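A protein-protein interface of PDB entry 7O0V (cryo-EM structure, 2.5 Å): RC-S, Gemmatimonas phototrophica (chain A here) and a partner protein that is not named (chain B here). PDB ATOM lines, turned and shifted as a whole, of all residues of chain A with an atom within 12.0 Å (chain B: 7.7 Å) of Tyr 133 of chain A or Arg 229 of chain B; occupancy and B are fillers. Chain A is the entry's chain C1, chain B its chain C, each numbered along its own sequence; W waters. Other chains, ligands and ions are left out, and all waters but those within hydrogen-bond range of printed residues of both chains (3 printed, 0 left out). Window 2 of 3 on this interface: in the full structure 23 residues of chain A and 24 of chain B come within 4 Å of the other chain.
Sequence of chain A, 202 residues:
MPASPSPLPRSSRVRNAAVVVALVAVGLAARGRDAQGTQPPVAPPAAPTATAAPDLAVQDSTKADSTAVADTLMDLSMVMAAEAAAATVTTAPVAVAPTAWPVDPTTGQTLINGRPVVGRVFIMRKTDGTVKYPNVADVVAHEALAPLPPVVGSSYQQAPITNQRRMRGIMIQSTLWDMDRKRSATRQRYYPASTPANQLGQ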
ATOM      1  N   LYS A 126      13.148   3.366 -32.011  1.00  0.00           N
ATOM      2  CA  LYS A 126      11.886   3.128 -32.694  1.00  0.00           C
ATOM      3  C   LYS A 126      10.806   4.068 -32.155  1.00  0.00           C
ATOM      4  O   LYS A 126      10.975   4.717 -31.120  1.00  0.00           O
ATOM      5  CB  LYS A 126      11.481   1.660 -32.572  1.00  0.00           C
ATOM      6  CG  LYS A 126      12.470   0.714 -33.251  1.00  0.00           C
ATOM      7  CD  LYS A 126      12.604   1.032 -34.737  1.00  0.00           C
ATOM      8  CE  LYS A 126      13.373  -0.042 -35.492  1.00  0.00           C
ATOM      9  NZ  LYS A 126      12.581  -1.281 -35.710  1.00  0.00           N
ATOM     10  N   THR A 127       9.694   4.148 -32.892  1.00  0.00           N
ATOM     11  CA  THR A 127       8.618   5.112 -32.667  1.00  0.00           C
ATOM     12  C   THR A 127       8.314   5.344 -31.190  1.00  0.00           C
ATOM     13  O   THR A 127       7.908   4.426 -30.472  1.00  0.00           O
ATOM     14  CB  THR A 127       7.349   4.634 -33.383  1.00  0.00           C
ATOM     15  OG1 THR A 127       7.624   4.440 -34.775  1.00  0.00           O
ATOM     16  CG2 THR A 127       6.231   5.652 -33.233  1.00  0.00           C
ATOM     17  N   ASP A 128       8.509   6.590 -30.750  1.00  0.00           N
ATOM     18  CA  ASP A 128       8.250   7.055 -29.386  1.00  0.00           C
ATOM     19  C   ASP A 128       9.014   6.269 -28.322  1.00  0.00           C
ATOM     20  O   ASP A 128       8.610   6.247 -27.157  1.00  0.00           O
ATOM     21  CB  ASP A 128       6.749   7.061 -29.074  1.00  0.00           C
ATOM     22  CG  ASP A 128       6.018   8.202 -29.761  1.00  0.00           C
ATOM     23  OD1 ASP A 128       6.063   9.337 -29.243  1.00  0.00           O
ATOM     24  OD2 ASP A 128       5.391   7.965 -30.813  1.00  0.00           O
ATOM     25  N   GLY A 129      10.117   5.621 -28.693  1.00  0.00           N
ATOM     26  CA  GLY A 129      10.887   4.843 -27.740  1.00  0.00           C
ATOM     27  C   GLY A 129      10.238   3.564 -27.263  1.00  0.00           C
ATOM     28  O   GLY A 129      10.672   3.004 -26.254  1.00  0.00           O
ATOM     29  N   THR A 130       9.202   3.090 -27.951  1.00  0.00           N
ATOM     30  CA  THR A 130       8.558   1.833 -27.588  1.00  0.00           C
ATOM     31  C   THR A 130       9.519   0.656 -27.724  1.00  0.00           C
ATOM     32  O   THR A 130      10.374   0.628 -28.614  1.00  0.00           O
ATOM     33  CB  THR A 130       7.315   1.601 -28.449  1.00  0.00           C
ATOM     34  OG1 THR A 130       7.635   1.816 -29.828  1.00  0.00           O
ATOM     35  CG2 THR A 130       6.205   2.551 -28.039  1.00  0.00           C
ATOM     36  N   VAL A 131       9.377  -0.317 -26.825  1.00  0.00           N
ATOM     37  CA  VAL A 131      10.176  -1.539 -26.834  1.00  0.00           C
ATOM     38  C   VAL A 131       9.244  -2.723 -26.605  1.00  0.00           C
ATOM     39  O   VAL A 131       8.372  -2.680 -25.734  1.00  0.00           O
ATOM     40  CB  VAL A 131      11.291  -1.515 -25.765  1.00  0.00           C
ATOM     41  CG1 VAL A 131      12.162  -2.757 -25.876  1.00  0.00           C
ATOM     42  CG2 VAL A 131      12.142  -0.261 -25.891  1.00  0.00           C
ATOM     43  N   LYS A 132       9.437  -3.778 -27.397  1.00  0.00           N
ATOM     44  CA  LYS A 132       8.671  -5.013 -27.270  1.00  0.00           C
ATOM     45  C   LYS A 132       8.752  -5.570 -25.850  1.00  0.00           C
ATOM     46  O   LYS A 132       9.817  -5.565 -25.227  1.00  0.00           O
ATOM     47  CB  LYS A 132       9.216  -6.018 -28.291  1.00  0.00           C
ATOM     48  CG  LYS A 132       8.374  -7.238 -28.601  1.00  0.00           C
ATOM     49  CD  LYS A 132       9.107  -8.082 -29.647  1.00  0.00           C
ATOM     50  CE  LYS A 132       8.296  -9.273 -30.128  1.00  0.00           C
ATOM     51  NZ  LYS A 132       8.367 -10.424 -29.188  1.00  0.00           N
ATOM     52  N   TYR A 133       7.620  -6.049 -25.336  1.00  0.00           N
ATOM     53  CA  TYR A 133       7.601  -6.686 -24.014  1.00  0.00           C
ATOM     54  C   TYR A 133       8.251  -8.064 -24.057  1.00  0.00           C
ATOM     55  O   TYR A 133       7.812  -8.921 -24.834  1.00  0.00           O
ATOM     56  CB  TYR A 133       6.170  -6.822 -23.490  1.00  0.00           C
ATOM     57  CG  TYR A 133       5.408  -5.531 -23.278  1.00  0.00           C
ATOM     58  CD1 TYR A 133       6.068  -4.317 -23.133  1.00  0.00           C
ATOM     59  CD2 TYR A 133       4.022  -5.533 -23.208  1.00  0.00           C
ATOM     60  CE1 TYR A 133       5.364  -3.144 -22.920  1.00  0.00           C
ATOM     61  CE2 TYR A 133       3.312  -4.368 -23.009  1.00  0.00           C
ATOM     62  CZ  TYR A 133       3.986  -3.176 -22.862  1.00  0.00           C
ATOM     63  OH  TYR A 133       3.277  -2.012 -22.677  1.00  0.00           O
ATOM     64  N   PRO A 134       9.288  -8.322 -23.251  1.00  0.00           N
ATOM     65  CA  PRO A 134      10.008  -9.604 -23.374  1.00  0.00           C
ATOM     66  C   PRO A 134       9.141 -10.817 -23.073  1.00  0.00           C
ATOM     67  O   PRO A 134       9.138 -11.786 -23.841  1.00  0.00           O
ATOM     68  CB  PRO A 134      11.154  -9.458 -22.361  1.00  0.00           C
ATOM     69  CG  PRO A 134      11.349  -7.994 -22.212  1.00  0.00           C
ATOM     70  CD  PRO A 134       9.978  -7.389 -22.347  1.00  0.00           C
ATOM     71  N   ASN A 135       8.399 -10.780 -21.969  1.00  0.00           N
ATOM     72  CA  ASN A 135       7.654 -11.925 -21.456  1.00  0.00           C
ATOM     73  C   ASN A 135       6.780 -11.438 -20.302  1.00  0.00           C
ATOM     74  O   ASN A 135       6.843 -10.273 -19.899  1.00  0.00           O
ATOM     75  CB  ASN A 135       8.592 -13.057 -21.028  1.00  0.00           C
ATOM     76  CG  ASN A 135       9.742 -12.569 -20.168  1.00  0.00           C
ATOM     77  OD1 ASN A 135       9.538 -12.001 -19.098  1.00  0.00           O
ATOM     78  ND2 ASN A 135      10.963 -12.786 -20.642  1.00  0.00           N
ATOM     79  N   VAL A 136       5.953 -12.347 -19.780  1.00  0.00           N
ATOM     80  CA  VAL A 136       5.076 -12.026 -18.655  1.00  0.00           C
ATOM     81  C   VAL A 136       5.874 -11.619 -17.420  1.00  0.00           C
ATOM     82  O   VAL A 136       5.520 -10.657 -16.728  1.00  0.00           O
ATOM     83  CB  VAL A 136       4.139 -13.213 -18.359  1.00  0.00           C
ATOM     84  CG1 VAL A 136       3.416 -13.015 -17.037  1.00  0.00           C
ATOM     85  CG2 VAL A 136       3.136 -13.378 -19.483  1.00  0.00           C
ATOM     86  N   ALA A 137       6.962 -12.334 -17.128  1.00  0.00           N
ATOM     87  CA  ALA A 137       7.749 -12.042 -15.932  1.00  0.00           C
ATOM     88  C   ALA A 137       8.308 -10.623 -15.932  1.00  0.00           C
ATOM     89  O   ALA A 137       8.341  -9.965 -14.885  1.00  0.00           O
ATOM     90  CB  ALA A 137       8.881 -13.060 -15.794  1.00  0.00           C
ATOM     91  N   ASP A 138       8.751 -10.129 -17.089  1.00  0.00           N
ATOM     92  CA  ASP A 138       9.193  -8.738 -17.176  1.00  0.00           C
ATOM     93  C   ASP A 138       8.049  -7.747 -16.985  1.00  0.00           C
ATOM     94  O   ASP A 138       8.221  -6.720 -16.318  1.00  0.00           O
ATOM     95  CB  ASP A 138       9.883  -8.487 -18.513  1.00  0.00           C
ATOM     96  CG  ASP A 138      10.479  -7.098 -18.603  1.00  0.00           C
ATOM     97  OD1 ASP A 138      11.612  -6.903 -18.116  1.00  0.00           O
ATOM     98  OD2 ASP A 138       9.810  -6.197 -19.148  1.00  0.00           O
ATOM     99  N   VAL A 139       6.881  -8.025 -17.566  1.00  0.00           N
ATOM    100  CA  VAL A 139       5.715  -7.168 -17.351  1.00  0.00           C
ATOM    101  C   VAL A 139       5.324  -7.136 -15.879  1.00  0.00           C
ATOM    102  O   VAL A 139       5.009  -6.076 -15.326  1.00  0.00           O
ATOM    103  CB  VAL A 139       4.547  -7.630 -18.243  1.00  0.00           C
ATOM    104  CG1 VAL A 139       3.245  -6.976 -17.810  1.00  0.00           C
ATOM    105  CG2 VAL A 139       4.845  -7.313 -19.698  1.00  0.00           C
ATOM    106  N   VAL A 140       5.350  -8.292 -15.216  1.00  0.00           N
ATOM    107  CA  VAL A 140       4.992  -8.364 -13.803  1.00  0.00           C
ATOM    108  C   VAL A 140       6.066  -7.744 -12.911  1.00  0.00           C
ATOM    109  O   VAL A 140       5.753  -7.192 -11.848  1.00  0.00           O
ATOM    110  CB  VAL A 140       4.703  -9.831 -13.429  1.00  0.00           C
ATOM    111  CG1 VAL A 140       4.534  -9.994 -11.928  1.00  0.00           C
ATOM    112  CG2 VAL A 140       3.465 -10.321 -14.161  1.00  0.00           C
ATOM    113  N   ALA A 141       7.333  -7.791 -13.327  1.00  0.00           N
ATOM    114  CA  ALA A 141       8.393  -7.130 -12.569  1.00  0.00           C
ATOM    115  C   ALA A 141       8.211  -5.616 -12.482  1.00  0.00           C
ATOM    116  O   ALA A 141       8.677  -4.997 -11.519  1.00  0.00           O
ATOM    117  CB  ALA A 141       9.753  -7.457 -13.184  1.00  0.00           C
ATOM    118  N   HIS A 142       7.554  -4.998 -13.463  1.00  0.00           N
ATOM    119  CA  HIS A 142       7.266  -3.570 -13.388  1.00  0.00           C
ATOM    120  C   HIS A 142       6.007  -3.227 -12.600  1.00  0.00           C
ATOM    121  O   HIS A 142       5.798  -2.049 -12.294  1.00  0.00           O
ATOM    122  CB  HIS A 142       7.162  -2.977 -14.794  1.00  0.00           C
ATOM    123  CG  HIS A 142       8.467  -2.932 -15.525  1.00  0.00           C
ATOM    124  ND1 HIS A 142       8.939  -3.983 -16.280  1.00  0.00           N
ATOM    125  CD2 HIS A 142       9.403  -1.958 -15.608  1.00  0.00           C
ATOM    126  CE1 HIS A 142      10.109  -3.658 -16.799  1.00  0.00           C
ATOM    127  NE2 HIS A 142      10.414  -2.434 -16.407  1.00  0.00           N
ATOM    128  N   GLU A 143       5.166  -4.199 -12.273  1.00  0.00           N
ATOM    129  CA  GLU A 143       3.942  -3.908 -11.544  1.00  0.00           C
ATOM    130  C   GLU A 143       4.189  -3.875 -10.036  1.00  0.00           C
ATOM    131  O   GLU A 143       5.283  -4.165  -9.549  1.00  0.00           O
ATOM    132  CB  GLU A 143       2.866  -4.933 -11.897  1.00  0.00           C
ATOM    133  CG  GLU A 143       2.320  -4.763 -13.307  1.00  0.00           C
ATOM    134  CD  GLU A 143       1.793  -3.363 -13.569  1.00  0.00           C
ATOM    135  OE1 GLU A 143       1.295  -2.720 -12.622  1.00  0.00           O
ATOM    136  OE2 GLU A 143       1.883  -2.900 -14.725  1.00  0.00           O
ATOM    137  N   ALA A 144       3.147  -3.505  -9.294  1.00  0.00           N
ATOM    138  CA  ALA A 144       3.109  -3.766  -7.863  1.00  0.00           C
ATOM    139  C   ALA A 144       3.196  -5.264  -7.580  1.00  0.00           C
ATOM    140  O   ALA A 144       2.954  -6.106  -8.448  1.00  0.00           O
ATOM    141  CB  ALA A 144       1.835  -3.189  -7.247  1.00  0.00           C
ATOM    142  N   LEU A 145       3.559  -5.590  -6.342  1.00  0.00           N
ATOM    143  CA  LEU A 145       3.530  -6.972  -5.888  1.00  0.00           C
ATOM    144  C   LEU A 145       2.103  -7.517  -5.933  1.00  0.00           C
ATOM    145  O   LEU A 145       1.127  -6.770  -6.022  1.00  0.00           O
ATOM    146  CB  LEU A 145       4.109  -7.069  -4.477  1.00  0.00           C
ATOM    147  CG  LEU A 145       5.557  -6.580  -4.354  1.00  0.00           C
ATOM    148  CD1 LEU A 145       6.072  -6.737  -2.935  1.00  0.00           C
ATOM    149  CD2 LEU A 145       6.466  -7.297  -5.343  1.00  0.00           C
ATOM    150  N   ASN B 221      -5.245   2.334 -17.944  1.00  0.00           N
ATOM    151  CA  ASN B 221      -5.369   1.827 -19.306  1.00  0.00           C
ATOM    152  C   ASN B 221      -6.275   0.605 -19.214  1.00  0.00           C
ATOM    153  O   ASN B 221      -5.886  -0.422 -18.650  1.00  0.00           O
ATOM    154  CB  ASN B 221      -4.002   1.490 -19.898  1.00  0.00           C
ATOM    155  CG  ASN B 221      -4.061   1.201 -21.389  1.00  0.00           C
ATOM    156  OD1 ASN B 221      -5.069   0.725 -21.903  1.00  0.00           O
ATOM    157  ND2 ASN B 221      -2.976   1.497 -22.089  1.00  0.00           N
ATOM    158  N   ARG B 223      -7.228  -1.704 -21.103  1.00  0.00           N
ATOM    159  CA  ARG B 223      -6.766  -3.011 -21.557  1.00  0.00           C
ATOM    160  C   ARG B 223      -6.228  -3.860 -20.411  1.00  0.00           C
ATOM    161  O   ARG B 223      -6.236  -5.092 -20.500  1.00  0.00           O
ATOM    162  CB  ARG B 223      -5.724  -2.850 -22.665  1.00  0.00           C
ATOM    163  CG  ARG B 223      -4.298  -2.649 -22.213  1.00  0.00           C
ATOM    164  CD  ARG B 223      -3.401  -2.505 -23.427  1.00  0.00           C
ATOM    165  NE  ARG B 223      -1.990  -2.412 -23.084  1.00  0.00           N
ATOM    166  CZ  ARG B 223      -1.001  -2.556 -23.954  1.00  0.00           C
ATOM    167  NH1 ARG B 223      -1.235  -2.745 -25.241  1.00  0.00           N
ATOM    168  NH2 ARG B 223       0.255  -2.491 -23.524  1.00  0.00           N
ATOM    169  N   GLN B 224      -5.757  -3.234 -19.330  1.00  0.00           N
ATOM    170  CA  GLN B 224      -5.378  -3.971 -18.120  1.00  0.00           C
ATOM    171  C   GLN B 224      -5.573  -3.058 -16.908  1.00  0.00           C
ATOM    172  O   GLN B 224      -4.684  -2.282 -16.553  1.00  0.00           O
ATOM    173  CB  GLN B 224      -3.949  -4.487 -18.212  1.00  0.00           C
ATOM    174  CG  GLN B 224      -3.473  -5.336 -17.027  1.00  0.00           C
ATOM    175  CD  GLN B 224      -4.138  -6.706 -16.892  1.00  0.00           C
ATOM    176  OE1 GLN B 224      -3.717  -7.514 -16.066  1.00  0.00           O
ATOM    177  NE2 GLN B 224      -5.150  -6.980 -17.705  1.00  0.00           N
ATOM    178  N   ALA B 226      -5.502  -3.734 -13.856  1.00  0.00           N
ATOM    179  CA  ALA B 226      -4.520  -3.986 -12.805  1.00  0.00           C
ATOM    180  C   ALA B 226      -3.203  -3.239 -12.991  1.00  0.00           C
ATOM    181  O   ALA B 226      -2.486  -3.041 -12.005  1.00  0.00           O
ATOM    182  CB  ALA B 226      -4.243  -5.486 -12.703  1.00  0.00           C
ATOM    183  N   SER B 227      -2.860  -2.823 -14.206  1.00  0.00           N
ATOM    184  CA  SER B 227      -1.533  -2.266 -14.448  1.00  0.00           C
ATOM    185  C   SER B 227      -1.373  -0.885 -13.821  1.00  0.00           C
ATOM    186  O   SER B 227      -2.261  -0.034 -13.911  1.00  0.00           O
ATOM    187  CB  SER B 227      -1.259  -2.187 -15.947  1.00  0.00           C
ATOM    188  OG  SER B 227       0.017  -1.628 -16.199  1.00  0.00           O
ATOM    189  N   TRP B 228      -0.221  -0.670 -13.182  1.00  0.00           N
ATOM    190  CA  TRP B 228       0.224   0.645 -12.731  1.00  0.00           C
ATOM    191  C   TRP B 228       1.153   1.327 -13.729  1.00  0.00           C
ATOM    192  O   TRP B 228       1.093   2.550 -13.893  1.00  0.00           O
ATOM    193  CB  TRP B 228       0.920   0.530 -11.374  1.00  0.00           C
ATOM    194  CG  TRP B 228       0.011   0.073 -10.279  1.00  0.00           C
ATOM    195  CD1 TRP B 228      -0.251  -1.214  -9.924  1.00  0.00           C
ATOM    196  CD2 TRP B 228      -0.765   0.897  -9.400  1.00  0.00           C
ATOM    197  NE1 TRP B 228      -1.140  -1.247  -8.879  1.00  0.00           N
ATOM    198  CE2 TRP B 228      -1.472   0.037  -8.539  1.00  0.00           C
ATOM    199  CE3 TRP B 228      -0.932   2.278  -9.259  1.00  0.00           C
ATOM    200  CZ2 TRP B 228      -2.328   0.511  -7.549  1.00  0.00           C
ATOM    201  CZ3 TRP B 228      -1.783   2.747  -8.274  1.00  0.00           C
ATOM    202  CH2 TRP B 228      -2.471   1.865  -7.433  1.00  0.00           C
ATOM    203  N   ARG B 229       2.023   0.556 -14.390  1.00  0.00           N
ATOM    204  CA  ARG B 229       2.938   1.126 -15.377  1.00  0.00           C
ATOM    205  C   ARG B 229       2.190   1.754 -16.547  1.00  0.00           C
ATOM    206  O   ARG B 229       2.583   2.813 -17.048  1.00  0.00           O
ATOM    207  CB  ARG B 229       3.902   0.055 -15.887  1.00  0.00           C
ATOM    208  CG  ARG B 229       4.843   0.567 -16.970  1.00  0.00           C
ATOM    209  CD  ARG B 229       5.955  -0.409 -17.310  1.00  0.00           C
ATOM    210  NE  ARG B 229       5.455  -1.627 -17.936  1.00  0.00           N
ATOM    211  CZ  ARG B 229       6.136  -2.348 -18.816  1.00  0.00           C
ATOM    212  NH1 ARG B 229       7.371  -2.028 -19.165  1.00  0.00           N
ATOM    213  NH2 ARG B 229       5.569  -3.424 -19.351  1.00  0.00           N
ATOM    214  N   GLU B 230       1.111   1.117 -16.995  1.00  0.00           N
ATOM    215  CA  GLU B 230       0.323   1.649 -18.099  1.00  0.00           C
ATOM    216  C   GLU B 230      -0.651   2.737 -17.668  1.00  0.00           C
ATOM    217  O   GLU B 230      -1.175   3.450 -18.528  1.00  0.00           O
ATOM    218  CB  GLU B 230      -0.427   0.508 -18.790  1.00  0.00           C
ATOM    219  CG  GLU B 230       0.503  -0.523 -19.411  1.00  0.00           C
ATOM    220  CD  GLU B 230      -0.224  -1.553 -20.251  1.00  0.00           C
ATOM    221  OE1 GLU B 230      -1.443  -1.398 -20.466  1.00  0.00           O
ATOM    222  OE2 GLU B 230       0.429  -2.518 -20.698  1.00  0.00           O
ATOM    223  N   ALA B 231      -0.910   2.878 -16.367  1.00  0.00           N
ATOM    224  CA  ALA B 231      -1.851   3.857 -15.844  1.00  0.00           C
ATOM    225  C   ALA B 231      -1.177   5.212 -15.642  1.00  0.00           C
ATOM    226  O   ALA B 231       0.019   5.279 -15.347  1.00  0.00           O
ATOM    227  CB  ALA B 231      -2.427   3.373 -14.520  1.00  0.00           C
ATOM    228  N   PRO B 232      -1.917   6.309 -15.800  1.00  0.00           N
ATOM    229  CA  PRO B 232      -1.395   7.629 -15.422  1.00  0.00           C
ATOM    230  C   PRO B 232      -1.008   7.684 -13.954  1.00  0.00           C
ATOM    231  O   PRO B 232      -1.496   6.886 -13.141  1.00  0.00           O
ATOM    232  CB  PRO B 232      -2.572   8.572 -15.728  1.00  0.00           C
ATOM    233  CG  PRO B 232      -3.371   7.836 -16.754  1.00  0.00           C
ATOM    234  CD  PRO B 232      -3.293   6.407 -16.305  1.00  0.00           C
ATOM    235  N   PRO B 233      -0.134   8.622 -13.577  1.00  0.00           N
ATOM    236  CA  PRO B 233       0.278   8.738 -12.167  1.00  0.00           C
ATOM    237  C   PRO B 233      -0.854   9.077 -11.208  1.00  0.00           C
ATOM    238  O   PRO B 233      -0.722   8.820 -10.005  1.00  0.00           O
ATOM    239  CB  PRO B 233       1.328   9.859 -12.202  1.00  0.00           C
ATOM    240  CG  PRO B 233       1.830   9.863 -13.605  1.00  0.00           C
ATOM    241  CD  PRO B 233       0.632   9.530 -14.444  1.00  0.00           C
ATOM    242  N   ARG B 235      -3.467   7.526 -10.664  1.00  0.00           N
ATOM    243  CA  ARG B 235      -3.888   6.326  -9.942  1.00  0.00           C
ATOM    244  C   ARG B 235      -3.182   6.186  -8.596  1.00  0.00           C
ATOM    245  O   ARG B 235      -3.783   5.719  -7.623  1.00  0.00           O
ATOM    246  CB  ARG B 235      -3.654   5.077 -10.791  1.00  0.00           C
ATOM    247  CG  ARG B 235      -4.484   3.901 -10.308  1.00  0.00           C
ATOM    248  CD  ARG B 235      -4.189   2.612 -11.041  1.00  0.00           C
ATOM    249  NE  ARG B 235      -4.913   1.510 -10.424  1.00  0.00           N
ATOM    250  CZ  ARG B 235      -4.550   0.237 -10.485  1.00  0.00           C
ATOM    251  NH1 ARG B 235      -3.600  -0.173 -11.307  1.00  0.00           N
ATOM    252  NH2 ARG B 235      -5.197  -0.656  -9.742  1.00  0.00           N
HETATM  253  O   HOH W   1       3.689  -3.587 -16.442  1.00  0.00           O
HETATM  254  O   HOH W   2      -0.415  -4.363 -11.206  1.00  0.00           O
HETATM  255  O   HOH W   3       9.079   0.012 -18.178  1.00  0.00           O
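Of the 12 printed residues of chain B, 6 touch a printed residue of chain A. Hydrophobic or aromatic side chains of chain B that line the printed part of chain A: Trp 228. Hydrophobic or aromatic side chains of chain A that line the printed part of chain B: Tyr 133, Val 139, His 142 and Ala 144. Among the printed residues, 10 pairs touch across the chains.
Tyr 133 of chain A touches three residues of chain B. Arg 229 of chain B touches just these residues of chain A: Tyr 133 (3.6 Å), Val 139 (3.97 Å), His 142 (3.8 Å) and Glu 143 (3.5 Å). Of chain A, only Tyr 133 (3.5 Å) comes within 4 Å of Glu 230 of chain B. No residue of chain A comes within 4 Å of Ala 231 of chain B. No residue of chain A comes within 4 Å of Pro 232 of chain B. Of the printed residues of chain A, Trp 228 of chain B touches Glu 143 and Ala 144. Of the printed residues of chain B, Val 139 of chain A touches Arg 229. Pro 233 of chain B touches none of the printed residues of chain A. Thr 127 of chain A touches none of the printed residues of chain B. The nearest residue of chain B that does not touch Tyr 133 of chain A is Asn 221 of chain B (7.2 Å). The nearest residue of chain A that does not touch Arg 229 of chain B is Asp 138 of chain A (4.8 Å).
CE1 of Tyr 133 of chain A touches NH2 of Arg 229 of chain B (3.6 Å). Tyr 133 of chain A touches Glu 230 of chain B (OH to OE2, 3.5 Å). Val 139 of chain A touches Arg 229 of chain B (CG2 to NH2, 3.97 Å). His 142 of chain A touches Arg 229 of chain B. Glu 143 of chain A touches Ala 226 of chain B. CB of Ala 144 of chain A touches NE1 of Trp 228 of chain B, 3.9 Å away.
The backbone NH (N) of Trp 228 of chain B is in hydrogen-bond range of the side-chain carboxylate (OE1) of Glu 143 of chain A. NH2 of Arg 223 of chain B sits at hydrogen-bond distance from OH of Tyr 133 of chain A. OG of Ser 227 of chain B lies within hydrogen-bond range of OE2 of Glu 143 of chain A (2.7 Å). The backbone NH of Arg 229 of chain B lies within hydrogen-bond range of the side-chain carboxylate of Glu 143 of chain A, at 3.5 Å.
OE2 of Glu 230 of chain B lies within salt-bridge range of NH2 of Arg 223 of chain B, at 2.8 Å. The backbone NH of Arg 223 of chain B lies close to the side-chain amide oxygen of Asn 221 of chain B (3.3 Å). The backbone carbonyl oxygen of Ser 227 of chain B lies within hydrogen-bond range of the guanidinium group of Arg 235 of chain B, at 2.9 Å. OG of Ser 227 of chain B sits at hydrogen-bond distance from N of Glu 230 of chain B (3.1 Å). The backbone carbonyl oxygen of Asp 138 of chain A is in hydrogen-bond range of a ring nitrogen (ND1) of His 142 of chain A. OG of Ser 227 of chain B sits at hydrogen-bond distance from N of Arg 229 of chain B.
Water W2 lies within hydrogen-bond range of the backbone carbonyl oxygen of Ala 226 of chain B (2.6 Å) and the side-chain carboxylate of Glu 143 of chain A (2.8 Å). Water W1 lies within hydrogen-bond range of OE2 of Glu 143 of chain A (2.6 Å), O of Val 139 of chain A (3.0 Å) and NE of Arg 229 of chain B (3.0 Å). Water W3 bridges NH1 of Arg 229 of chain B (2.8 Å) and NE2 of His 142 of chain A (3.3 Å).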
